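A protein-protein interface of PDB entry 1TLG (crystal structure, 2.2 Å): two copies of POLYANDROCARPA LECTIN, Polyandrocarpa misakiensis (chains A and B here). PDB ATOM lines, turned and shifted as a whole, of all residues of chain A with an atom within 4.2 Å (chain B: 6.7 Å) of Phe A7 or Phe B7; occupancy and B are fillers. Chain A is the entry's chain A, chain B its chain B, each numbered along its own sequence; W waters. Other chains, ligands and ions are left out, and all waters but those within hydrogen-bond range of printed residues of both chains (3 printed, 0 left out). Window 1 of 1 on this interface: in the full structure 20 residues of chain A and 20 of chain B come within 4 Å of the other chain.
Water W2 lies within hydrogen-bond range of the side-chain carboxylate (OE2) of Glu A4, the side-chain hydroxyl (OG) of Ser B8 and the side-chain hydroxyl (OH) of Tyr B20.
Water W3 lies within hydrogen-bond range of OE2 of Glu B4 and OG of Ser A8.
Water W1 lies within hydrogen-bond range of the backbone carbonyl oxygen (O) of Tyr A3 (2.8 Å) and the backbone carbonyl oxygen (O) of Phe B7 (3.2 Å).
Glu A4 touches Ser B8, and with the chains exchanged Ser A8 touches Glu B4.
Ile A5 touches its own counterpart, Ile B5.
Ile A5 touches Leu B6, and with the chains exchanged Leu A6 touches Ile B5.
Ile A5 touches Phe B7, and with the chains exchanged Phe A7 touches Ile B5.
Of the 19 pairs that touch across the chains among the printed residues, 14 have their exchanged pair printed and touching as well.
N of Ile A5 is in hydrogen-bond range of O of Phe B7 (2.8 Å).
The side-chain carboxylate (OE2) of Glu A4 lies within hydrogen-bond range of the side-chain hydroxyl (OH) of Tyr B20, 2.7 Å away.
The backbone NH of Tyr A3 sits at hydrogen-bond distance from the side-chain carboxylate of Asp B9 (2.9 Å).
The backbone carbonyl oxygen of Phe A7 lies within hydrogen-bond range of the backbone NH of Ile B5 (2.8 Å).
Phe A7 touches just these residues of chain B: Glu B4, Ile B5, Phe B7 and Phe B45.
Of the printed residues of chain A, Tyr B3 touches Ser A8 (3.8 Å).
Printed residues of chain A within 4 Å of Glu B4: Phe A7 (3.3 Å) and Ser A8 (3.8 Å).
Of the printed residues of chain A, Leu B6 touches Ile A5 (3.3 Å).
Phe B7 touches five residues of chain A.
Printed residues of chain A within 4 Å of Ala B41: Phe A45 (3.3 Å).
Ile B42 touches none of the printed residues of chain A.
Leu B43 touches none of the printed residues of chain A.
The nearest residue of chain B that does not touch Phe A7 is Tyr B3 (4.03 Å).
The nearest printed residue of chain A that does not touch Phe B7 is Leu A6 (5.1 Å).
The nearest printed residue of chain A that does not touch Ile B5 is Phe A45 (4.5 Å).
The backbone carbonyl oxygen of Val A117 lies within hydrogen-bond range of the backbone NH of Ser A8.
The backbone carbonyl oxygen (O) of Leu B6 lies within hydrogen-bond range of the backbone NH (N) of Cys B119 (2.8 Å).
N of Glu B10 is in hydrogen-bond range of OG of Ser B8 (2.9 Å).
The backbone carbonyl oxygen of Val B117 is in hydrogen-bond range of the backbone NH of Ser B8.
Hydrophobic or aromatic side chains of chain A within 4 Å of the printed part of chain B: Leu A6, Phe A7 and Phe A45.
Among the printed residues, no Asp or Glu carboxylate lies within 4 Å of a Lys or Arg side-chain nitrogen of the other chain.
Among the printed residues, pairs that only touch across the chains: Glu A4 with Phe B7 (3.2 Å), Phe A45 with Ala B41 (3.3 Å), Phe A7 with Glu B4 (3.3 Å), Ile A5 with Leu B6 (3.3 Å), Leu A6 with Ile B5 (3.4 Å), Phe A7 with Phe B7 (3.5 Å), Ile A5 with Ile B5 (3.6 Å), Ser A8 with Glu B4 (3.8 Å), Ser A8 with Tyr B3 (3.8 Å), Tyr A3 with Phe B7 (3.9 Å), Ser A8 with Leu B123 (3.9 Å), Phe A7 with Phe B45 (3.9 Å), Phe A45 with Phe B7 (3.9 Å), Glu A4 with Ser B8 (3.97 Å) and Tyr A3 with Ser B8 (3.98 Å).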
ATOM      1  N   TYR A   3      23.599  12.404  27.481  1.00  0.00           N
ATOM      2  CA  TYR A   3      22.202  12.241  27.128  1.00  0.00           C
ATOM      3  C   TYR A   3      21.446  11.118  27.815  1.00  0.00           C
ATOM      4  O   TYR A   3      21.995  10.164  28.336  1.00  0.00           O
ATOM      5  CB  TYR A   3      22.160  11.839  25.635  1.00  0.00           C
ATOM      6  CG  TYR A   3      22.741  12.800  24.639  1.00  0.00           C
ATOM      7  CD1 TYR A   3      24.096  12.765  24.315  1.00  0.00           C
ATOM      8  CD2 TYR A   3      21.935  13.742  24.005  1.00  0.00           C
ATOM      9  CE1 TYR A   3      24.641  13.637  23.401  1.00  0.00           C
ATOM     10  CE2 TYR A   3      22.480  14.620  23.082  1.00  0.00           C
ATOM     11  CZ  TYR A   3      23.819  14.567  22.783  1.00  0.00           C
ATOM     12  OH  TYR A   3      24.349  15.444  21.862  1.00  0.00           O
ATOM     13  N   GLU A   4      20.130  11.230  27.721  1.00  0.00           N
ATOM     14  CA  GLU A   4      19.193  10.169  28.039  1.00  0.00           C
ATOM     15  C   GLU A   4      18.821   9.657  26.631  1.00  0.00           C
ATOM     16  O   GLU A   4      18.672  10.500  25.728  1.00  0.00           O
ATOM     17  CB  GLU A   4      17.947  10.587  28.772  1.00  0.00           C
ATOM     18  CG  GLU A   4      18.080  10.943  30.238  1.00  0.00           C
ATOM     19  CD  GLU A   4      16.814  11.589  30.767  1.00  0.00           C
ATOM     20  OE1 GLU A   4      15.951  11.920  29.931  1.00  0.00           O
ATOM     21  OE2 GLU A   4      16.648  11.750  31.989  1.00  0.00           O
ATOM     22  N   ILE A   5      18.837   8.363  26.402  1.00  0.00           N
ATOM     23  CA  ILE A   5      18.487   7.843  25.077  1.00  0.00           C
ATOM     24  C   ILE A   5      17.373   6.809  25.275  1.00  0.00           C
ATOM     25  O   ILE A   5      17.475   5.908  26.112  1.00  0.00           O
ATOM     26  CB  ILE A   5      19.641   7.220  24.289  1.00  0.00           C
ATOM     27  CG1 ILE A   5      20.798   8.181  24.037  1.00  0.00           C
ATOM     28  CG2 ILE A   5      19.173   6.620  22.971  1.00  0.00           C
ATOM     29  CD1 ILE A   5      20.553   9.376  23.141  1.00  0.00           C
ATOM     30  N   LEU A   6      16.290   6.992  24.541  1.00  0.00           N
ATOM     31  CA  LEU A   6      15.166   6.066  24.612  1.00  0.00           C
ATOM     32  C   LEU A   6      15.009   5.302  23.307  1.00  0.00           C
ATOM     33  O   LEU A   6      14.873   5.904  22.251  1.00  0.00           O
ATOM     34  CB  LEU A   6      13.865   6.815  24.939  1.00  0.00           C
ATOM     35  CG  LEU A   6      12.588   5.963  24.889  1.00  0.00           C
ATOM     36  CD1 LEU A   6      12.565   4.876  25.958  1.00  0.00           C
ATOM     37  CD2 LEU A   6      11.354   6.839  25.058  1.00  0.00           C
ATOM     38  N   PHE A   7      15.010   3.987  23.330  1.00  0.00           N
ATOM     39  CA  PHE A   7      14.760   3.154  22.165  1.00  0.00           C
ATOM     40  C   PHE A   7      13.385   2.509  22.379  1.00  0.00           C
ATOM     41  O   PHE A   7      13.142   2.016  23.482  1.00  0.00           O
ATOM     42  CB  PHE A   7      15.748   2.012  21.969  1.00  0.00           C
ATOM     43  CG  PHE A   7      17.178   2.409  21.789  1.00  0.00           C
ATOM     44  CD1 PHE A   7      18.011   2.536  22.890  1.00  0.00           C
ATOM     45  CD2 PHE A   7      17.686   2.645  20.523  1.00  0.00           C
ATOM     46  CE1 PHE A   7      19.340   2.886  22.714  1.00  0.00           C
ATOM     47  CE2 PHE A   7      19.013   3.001  20.345  1.00  0.00           C
ATOM     48  CZ  PHE A   7      19.831   3.122  21.446  1.00  0.00           C
ATOM     49  N   SER A   8      12.545   2.503  21.366  1.00  0.00           N
ATOM     50  CA  SER A   8      11.235   1.888  21.484  1.00  0.00           C
ATOM     51  C   SER A   8      10.951   0.944  20.322  1.00  0.00           C
ATOM     52  O   SER A   8      11.113   1.326  19.166  1.00  0.00           O
ATOM     53  CB  SER A   8      10.112   2.927  21.539  1.00  0.00           C
ATOM     54  OG  SER A   8       8.885   2.207  21.411  1.00  0.00           O
ATOM     55  N   ILE A  42      24.643   4.168  19.951  1.00  0.00           N
ATOM     56  CA  ILE A  42      23.292   4.071  19.390  1.00  0.00           C
ATOM     57  C   ILE A  42      23.249   3.048  18.259  1.00  0.00           C
ATOM     58  O   ILE A  42      22.330   2.237  18.233  1.00  0.00           O
ATOM     59  CB  ILE A  42      22.772   5.439  18.923  1.00  0.00           C
ATOM     60  CG1 ILE A  42      22.409   6.275  20.156  1.00  0.00           C
ATOM     61  CG2 ILE A  42      21.577   5.310  17.991  1.00  0.00           C
ATOM     62  CD1 ILE A  42      22.259   7.761  19.871  1.00  0.00           C
ATOM     63  N   PHE A  45      23.399  -0.748  19.271  1.00  0.00           N
ATOM     64  CA  PHE A  45      22.086  -1.230  19.683  1.00  0.00           C
ATOM     65  C   PHE A  45      21.246  -1.588  18.456  1.00  0.00           C
ATOM     66  O   PHE A  45      20.742  -2.697  18.343  1.00  0.00           O
ATOM     67  CB  PHE A  45      21.367  -0.187  20.547  1.00  0.00           C
ATOM     68  CG  PHE A  45      20.089  -0.595  21.215  1.00  0.00           C
ATOM     69  CD1 PHE A  45      18.895  -0.684  20.504  1.00  0.00           C
ATOM     70  CD2 PHE A  45      20.053  -0.894  22.569  1.00  0.00           C
ATOM     71  CE1 PHE A  45      17.710  -1.060  21.114  1.00  0.00           C
ATOM     72  CE2 PHE A  45      18.865  -1.270  23.180  1.00  0.00           C
ATOM     73  CZ  PHE A  45      17.689  -1.360  22.459  1.00  0.00           C
ATOM     74  N   THR A  46      21.062  -0.636  17.549  1.00  0.00           N
ATOM     75  CA  THR A  46      20.233  -0.860  16.362  1.00  0.00           C
ATOM     76  C   THR A  46      20.810  -1.954  15.479  1.00  0.00           C
ATOM     77  O   THR A  46      20.059  -2.695  14.853  1.00  0.00           O
ATOM     78  CB  THR A  46      20.031   0.436  15.562  1.00  0.00           C
ATOM     79  OG1 THR A  46      21.287   0.849  15.012  1.00  0.00           O
ATOM     80  CG2 THR A  46      19.511   1.544  16.460  1.00  0.00           C
ATOM     81  N   VAL A 117      11.428   3.837  17.051  1.00  0.00           N
ATOM     82  CA  VAL A 117      11.769   5.164  17.496  1.00  0.00           C
ATOM     83  C   VAL A 117      12.931   5.260  18.473  1.00  0.00           C
ATOM     84  O   VAL A 117      13.087   4.463  19.397  1.00  0.00           O
ATOM     85  CB  VAL A 117      10.520   5.755  18.204  1.00  0.00           C
ATOM     86  CG1 VAL A 117      10.709   7.231  18.532  1.00  0.00           C
ATOM     87  CG2 VAL A 117       9.277   5.558  17.318  1.00  0.00           C
ATOM     88  N   ILE A 118      13.703   6.321  18.320  1.00  0.00           N
ATOM     89  CA  ILE A 118      14.811   6.689  19.173  1.00  0.00           C
ATOM     90  C   ILE A 118      14.631   8.142  19.606  1.00  0.00           C
ATOM     91  O   ILE A 118      14.589   9.012  18.724  1.00  0.00           O
ATOM     92  CB  ILE A 118      16.170   6.591  18.451  1.00  0.00           C
ATOM     93  CG1 ILE A 118      16.292   5.243  17.752  1.00  0.00           C
ATOM     94  CG2 ILE A 118      17.313   6.822  19.440  1.00  0.00           C
ATOM     95  CD1 ILE A 118      17.643   4.940  17.153  1.00  0.00           C
ATOM     96  N   TYR B   3      10.182  -4.106  24.008  1.00  0.00           N
ATOM     97  CA  TYR B   3      10.381  -3.133  25.062  1.00  0.00           C
ATOM     98  C   TYR B   3      10.659  -1.708  24.593  1.00  0.00           C
ATOM     99  O   TYR B   3      11.017  -1.404  23.463  1.00  0.00           O
ATOM    100  CB  TYR B   3      11.643  -3.537  25.874  1.00  0.00           C
ATOM    101  CG  TYR B   3      11.573  -4.800  26.681  1.00  0.00           C
ATOM    102  CD1 TYR B   3      11.926  -6.024  26.122  1.00  0.00           C
ATOM    103  CD2 TYR B   3      11.160  -4.791  28.015  1.00  0.00           C
ATOM    104  CE1 TYR B   3      11.868  -7.192  26.855  1.00  0.00           C
ATOM    105  CE2 TYR B   3      11.105  -5.960  28.753  1.00  0.00           C
ATOM    106  CZ  TYR B   3      11.450  -7.156  28.168  1.00  0.00           C
ATOM    107  OH  TYR B   3      11.394  -8.327  28.889  1.00  0.00           O
ATOM    108  N   GLU B   4      10.557  -0.817  25.558  1.00  0.00           N
ATOM    109  CA  GLU B   4      11.016   0.547  25.570  1.00  0.00           C
ATOM    110  C   GLU B   4      12.263   0.467  26.496  1.00  0.00           C
ATOM    111  O   GLU B   4      12.113  -0.128  27.575  1.00  0.00           O
ATOM    112  CB  GLU B   4      10.074   1.574  26.170  1.00  0.00           C
ATOM    113  CG  GLU B   4       8.966   2.054  25.245  1.00  0.00           C
ATOM    114  CD  GLU B   4       8.014   3.013  25.929  1.00  0.00           C
ATOM    115  OE1 GLU B   4       8.058   3.120  27.168  1.00  0.00           O
ATOM    116  OE2 GLU B   4       7.211   3.675  25.231  1.00  0.00           O
ATOM    117  N   ILE B   5      13.410   0.952  26.061  1.00  0.00           N
ATOM    118  CA  ILE B   5      14.609   0.879  26.892  1.00  0.00           C
ATOM    119  C   ILE B   5      15.191   2.298  26.994  1.00  0.00           C
ATOM    120  O   ILE B   5      15.422   2.955  25.974  1.00  0.00           O
ATOM    121  CB  ILE B   5      15.694  -0.081  26.375  1.00  0.00           C
ATOM    122  CG1 ILE B   5      15.240  -1.532  26.251  1.00  0.00           C
ATOM    123  CG2 ILE B   5      16.948  -0.021  27.251  1.00  0.00           C
ATOM    124  CD1 ILE B   5      14.848  -2.267  27.516  1.00  0.00           C
ATOM    125  N   LEU B   6      15.411   2.753  28.223  1.00  0.00           N
ATOM    126  CA  LEU B   6      15.966   4.078  28.464  1.00  0.00           C
ATOM    127  C   LEU B   6      17.335   4.009  29.146  1.00  0.00           C
ATOM    128  O   LEU B   6      17.480   3.443  30.231  1.00  0.00           O
ATOM    129  CB  LEU B   6      14.993   4.873  29.334  1.00  0.00           C
ATOM    130  CG  LEU B   6      15.464   6.205  29.906  1.00  0.00           C
ATOM    131  CD1 LEU B   6      15.521   7.315  28.861  1.00  0.00           C
ATOM    132  CD2 LEU B   6      14.552   6.611  31.055  1.00  0.00           C
ATOM    133  N   PHE B   7      18.327   4.629  28.524  1.00  0.00           N
ATOM    134  CA  PHE B   7      19.677   4.725  29.048  1.00  0.00           C
ATOM    135  C   PHE B   7      19.935   6.174  29.495  1.00  0.00           C
ATOM    136  O   PHE B   7      19.670   7.114  28.734  1.00  0.00           O
ATOM    137  CB  PHE B   7      20.755   4.388  28.019  1.00  0.00           C
ATOM    138  CG  PHE B   7      20.796   2.997  27.466  1.00  0.00           C
ATOM    139  CD1 PHE B   7      21.538   2.006  28.098  1.00  0.00           C
ATOM    140  CD2 PHE B   7      20.116   2.677  26.311  1.00  0.00           C
ATOM    141  CE1 PHE B   7      21.592   0.728  27.586  1.00  0.00           C
ATOM    142  CE2 PHE B   7      20.159   1.399  25.786  1.00  0.00           C
ATOM    143  CZ  PHE B   7      20.889   0.426  26.429  1.00  0.00           C
ATOM    144  N   SER B   8      20.459   6.354  30.700  1.00  0.00           N
ATOM    145  CA  SER B   8      20.772   7.676  31.197  1.00  0.00           C
ATOM    146  C   SER B   8      22.235   7.799  31.623  1.00  0.00           C
ATOM    147  O   SER B   8      22.714   6.986  32.415  1.00  0.00           O
ATOM    148  CB  SER B   8      19.947   8.090  32.425  1.00  0.00           C
ATOM    149  OG  SER B   8      20.512   9.312  32.920  1.00  0.00           O
ATOM    150  N   ASP B   9      22.879   8.854  31.141  1.00  0.00           N
ATOM    151  CA  ASP B   9      24.250   9.148  31.517  1.00  0.00           C
ATOM    152  C   ASP B   9      24.341   9.720  32.934  1.00  0.00           C
ATOM    153  O   ASP B   9      25.441   9.831  33.480  1.00  0.00           O
ATOM    154  CB  ASP B   9      24.858  10.142  30.535  1.00  0.00           C
ATOM    155  CG  ASP B   9      25.404   9.503  29.281  1.00  0.00           C
ATOM    156  OD1 ASP B   9      25.999   8.401  29.322  1.00  0.00           O
ATOM    157  OD2 ASP B   9      25.225  10.138  28.225  1.00  0.00           O
ATOM    158  N   GLU B  10      23.228  10.133  33.524  1.00  0.00           N
ATOM    159  CA  GLU B  10      23.301  10.687  34.882  1.00  0.00           C
ATOM    160  C   GLU B  10      23.517   9.566  35.896  1.00  0.00           C
ATOM    161  O   GLU B  10      22.936   8.492  35.753  1.00  0.00           O
ATOM    162  CB  GLU B  10      22.080  11.535  35.209  1.00  0.00           C
ATOM    163  CG  GLU B  10      22.121  12.192  36.586  1.00  0.00           C
ATOM    164  CD  GLU B  10      23.338  13.088  36.768  1.00  0.00           C
ATOM    165  OE1 GLU B  10      23.271  14.293  36.438  1.00  0.00           O
ATOM    166  OE2 GLU B  10      24.383  12.578  37.234  1.00  0.00           O
ATOM    167  N   TYR B  20      14.039   6.786  39.954  1.00  0.00           N
ATOM    168  CA  TYR B  20      14.185   7.472  38.672  1.00  0.00           C
ATOM    169  C   TYR B  20      13.370   6.756  37.592  1.00  0.00           C
ATOM    170  O   TYR B  20      12.617   7.410  36.886  1.00  0.00           O
ATOM    171  CB  TYR B  20      15.657   7.579  38.276  1.00  0.00           C
ATOM    172  CG  TYR B  20      15.935   8.031  36.861  1.00  0.00           C
ATOM    173  CD1 TYR B  20      15.974   7.112  35.816  1.00  0.00           C
ATOM    174  CD2 TYR B  20      16.161   9.361  36.551  1.00  0.00           C
ATOM    175  CE1 TYR B  20      16.211   7.507  34.515  1.00  0.00           C
ATOM    176  CE2 TYR B  20      16.408   9.763  35.250  1.00  0.00           C
ATOM    177  CZ  TYR B  20      16.426   8.835  34.233  1.00  0.00           C
ATOM    178  OH  TYR B  20      16.671   9.231  32.940  1.00  0.00           O
ATOM    179  N   MET B  26       8.549   3.499  34.221  1.00  0.00           N
ATOM    180  CA  MET B  26       9.348   2.340  33.818  1.00  0.00           C
ATOM    181  C   MET B  26       9.920   1.639  35.047  1.00  0.00           C
ATOM    182  O   MET B  26       9.601   1.971  36.191  1.00  0.00           O
ATOM    183  CB  MET B  26      10.450   2.797  32.852  1.00  0.00           C
ATOM    184  CG  MET B  26       9.988   3.789  31.787  1.00  0.00           C
ATOM    185  SD  MET B  26      11.294   4.419  30.710  1.00  0.00           S
ATOM    186  CE  MET B  26      11.742   2.896  29.866  1.00  0.00           C
ATOM    187  N   ALA B  41      21.365  -6.407  22.608  1.00  0.00           N
ATOM    188  CA  ALA B  41      21.302  -5.025  22.197  1.00  0.00           C
ATOM    189  C   ALA B  41      21.707  -4.089  23.341  1.00  0.00           C
ATOM    190  O   ALA B  41      22.443  -3.127  23.091  1.00  0.00           O
ATOM    191  CB  ALA B  41      19.928  -4.623  21.668  1.00  0.00           C
ATOM    192  N   ILE B  42      21.237  -4.354  24.550  1.00  0.00           N
ATOM    193  CA  ILE B  42      21.570  -3.512  25.690  1.00  0.00           C
ATOM    194  C   ILE B  42      23.082  -3.505  25.925  1.00  0.00           C
ATOM    195  O   ILE B  42      23.680  -2.452  26.087  1.00  0.00           O
ATOM    196  CB  ILE B  42      20.851  -3.981  26.974  1.00  0.00           C
ATOM    197  CG1 ILE B  42      19.334  -3.828  26.802  1.00  0.00           C
ATOM    198  CG2 ILE B  42      21.344  -3.227  28.209  1.00  0.00           C
ATOM    199  CD1 ILE B  42      18.530  -4.399  27.958  1.00  0.00           C
ATOM    200  N   LEU B  43      23.679  -4.688  25.976  1.00  0.00           N
ATOM    201  CA  LEU B  43      25.107  -4.814  26.214  1.00  0.00           C
ATOM    202  C   LEU B  43      25.962  -4.279  25.071  1.00  0.00           C
ATOM    203  O   LEU B  43      27.078  -3.844  25.358  1.00  0.00           O
ATOM    204  CB  LEU B  43      25.462  -6.272  26.524  1.00  0.00           C
ATOM    205  CG  LEU B  43      24.924  -6.787  27.874  1.00  0.00           C
ATOM    206  CD1 LEU B  43      25.185  -8.277  27.986  1.00  0.00           C
ATOM    207  CD2 LEU B  43      25.550  -6.030  29.043  1.00  0.00           C
ATOM    208  N   PHE B  45      25.304  -1.560  23.464  1.00  0.00           N
ATOM    209  CA  PHE B  45      25.326  -0.137  23.778  1.00  0.00           C
ATOM    210  C   PHE B  45      26.322   0.145  24.919  1.00  0.00           C
ATOM    211  O   PHE B  45      27.171   1.047  24.803  1.00  0.00           O
ATOM    212  CB  PHE B  45      23.923   0.314  24.163  1.00  0.00           C
ATOM    213  CG  PHE B  45      23.716   1.784  24.400  1.00  0.00           C
ATOM    214  CD1 PHE B  45      24.008   2.352  25.625  1.00  0.00           C
ATOM    215  CD2 PHE B  45      23.188   2.591  23.405  1.00  0.00           C
ATOM    216  CE1 PHE B  45      23.790   3.704  25.856  1.00  0.00           C
ATOM    217  CE2 PHE B  45      22.975   3.944  23.637  1.00  0.00           C
ATOM    218  CZ  PHE B  45      23.272   4.515  24.863  1.00  0.00           C
ATOM    219  N   THR B  46      26.177  -0.600  26.017  1.00  0.00           N
ATOM    220  CA  THR B  46      27.043  -0.391  27.176  1.00  0.00           C
ATOM    221  C   THR B  46      28.500  -0.706  26.862  1.00  0.00           C
ATOM    222  O   THR B  46      29.410  -0.096  27.426  1.00  0.00           O
ATOM    223  CB  THR B  46      26.592  -1.171  28.429  1.00  0.00           C
ATOM    224  OG1 THR B  46      26.551  -2.580  28.221  1.00  0.00           O
ATOM    225  CG2 THR B  46      25.181  -0.693  28.819  1.00  0.00           C
ATOM    226  N   TYR B  53      26.745   0.518  34.839  1.00  0.00           N
ATOM    227  CA  TYR B  53      25.319   0.824  34.859  1.00  0.00           C
ATOM    228  C   TYR B  53      24.607  -0.054  35.895  1.00  0.00           C
ATOM    229  O   TYR B  53      24.948  -1.238  36.029  1.00  0.00           O
ATOM    230  CB  TYR B  53      24.619   0.538  33.532  1.00  0.00           C
ATOM    231  CG  TYR B  53      24.969   1.446  32.379  1.00  0.00           C
ATOM    232  CD1 TYR B  53      26.202   1.342  31.753  1.00  0.00           C
ATOM    233  CD2 TYR B  53      24.073   2.407  31.924  1.00  0.00           C
ATOM    234  CE1 TYR B  53      26.533   2.176  30.704  1.00  0.00           C
ATOM    235  CE2 TYR B  53      24.386   3.238  30.865  1.00  0.00           C
ATOM    236  CZ  TYR B  53      25.616   3.121  30.265  1.00  0.00           C
ATOM    237  OH  TYR B  53      25.960   3.923  29.214  1.00  0.00           O
ATOM    238  N   ILE B  99      26.102  -3.640  35.763  1.00  0.00           N
ATOM    239  CA  ILE B  99      26.829  -4.028  34.575  1.00  0.00           C
ATOM    240  C   ILE B  99      28.180  -3.314  34.816  1.00  0.00           C
ATOM    241  O   ILE B  99      28.205  -2.086  34.798  1.00  0.00           O
ATOM    242  CB  ILE B  99      26.233  -3.553  33.252  1.00  0.00           C
ATOM    243  CG1 ILE B  99      24.903  -4.253  32.942  1.00  0.00           C
ATOM    244  CG2 ILE B  99      27.194  -3.736  32.087  1.00  0.00           C
ATOM    245  CD1 ILE B  99      24.168  -3.651  31.757  1.00  0.00           C
ATOM    246  N   VAL B 117      22.083   4.655  34.654  1.00  0.00           N
ATOM    247  CA  VAL B 117      20.825   3.943  34.781  1.00  0.00           C
ATOM    248  C   VAL B 117      20.253   3.428  33.469  1.00  0.00           C
ATOM    249  O   VAL B 117      20.291   4.082  32.430  1.00  0.00           O
ATOM    250  CB  VAL B 117      19.779   4.871  35.454  1.00  0.00           C
ATOM    251  CG1 VAL B 117      18.484   4.149  35.785  1.00  0.00           C
ATOM    252  CG2 VAL B 117      20.360   5.477  36.731  1.00  0.00           C
ATOM    253  N   ILE B 118      19.654   2.246  33.582  1.00  0.00           N
ATOM    254  CA  ILE B 118      18.930   1.628  32.487  1.00  0.00           C
ATOM    255  C   ILE B 118      17.518   1.248  32.957  1.00  0.00           C
ATOM    256  O   ILE B 118      17.343   0.430  33.874  1.00  0.00           O
ATOM    257  CB  ILE B 118      19.624   0.389  31.907  1.00  0.00           C
ATOM    258  CG1 ILE B 118      21.109   0.662  31.671  1.00  0.00           C
ATOM    259  CG2 ILE B 118      18.940  -0.034  30.605  1.00  0.00           C
ATOM    260  CD1 ILE B 118      21.906  -0.573  31.316  1.00  0.00           C
ATOM    261  N   CYS B 119      16.517   1.832  32.315  1.00  0.00           N
ATOM    262  CA  CYS B 119      15.132   1.523  32.600  1.00  0.00           C
ATOM    263  C   CYS B 119      14.495   0.736  31.447  1.00  0.00           C
ATOM    264  O   CYS B 119      14.922   0.842  30.295  1.00  0.00           O
ATOM    265  CB  CYS B 119      14.303   2.785  32.845  1.00  0.00           C
ATOM    266  SG  CYS B 119      15.026   4.004  33.962  1.00  0.00           S
ATOM    267  N   LEU B 123       6.562  -3.831  26.290  1.00  0.00           N
ATOM    268  CA  LEU B 123       5.570  -3.248  25.390  1.00  0.00           C
ATOM    269  C   LEU B 123       4.360  -4.147  25.185  1.00  0.00           C
ATOM    270  O   LEU B 123       4.426  -5.355  25.041  1.00  0.00           O
ATOM    271  CB  LEU B 123       6.149  -2.774  24.060  1.00  0.00           C
ATOM    272  CG  LEU B 123       6.963  -1.474  24.159  1.00  0.00           C
ATOM    273  CD1 LEU B 123       7.623  -1.154  22.825  1.00  0.00           C
ATOM    274  CD2 LEU B 123       6.072  -0.330  24.622  1.00  0.00           C
HETATM  275  O   HOH W   1      22.577   7.633  27.380  1.00  0.00           O
HETATM  276  O   HOH W   2      18.593  11.156  33.554  1.00  0.00           O
HETATM  277  O   HOH W   3       6.644   2.811  22.800  1.00  0.00           O
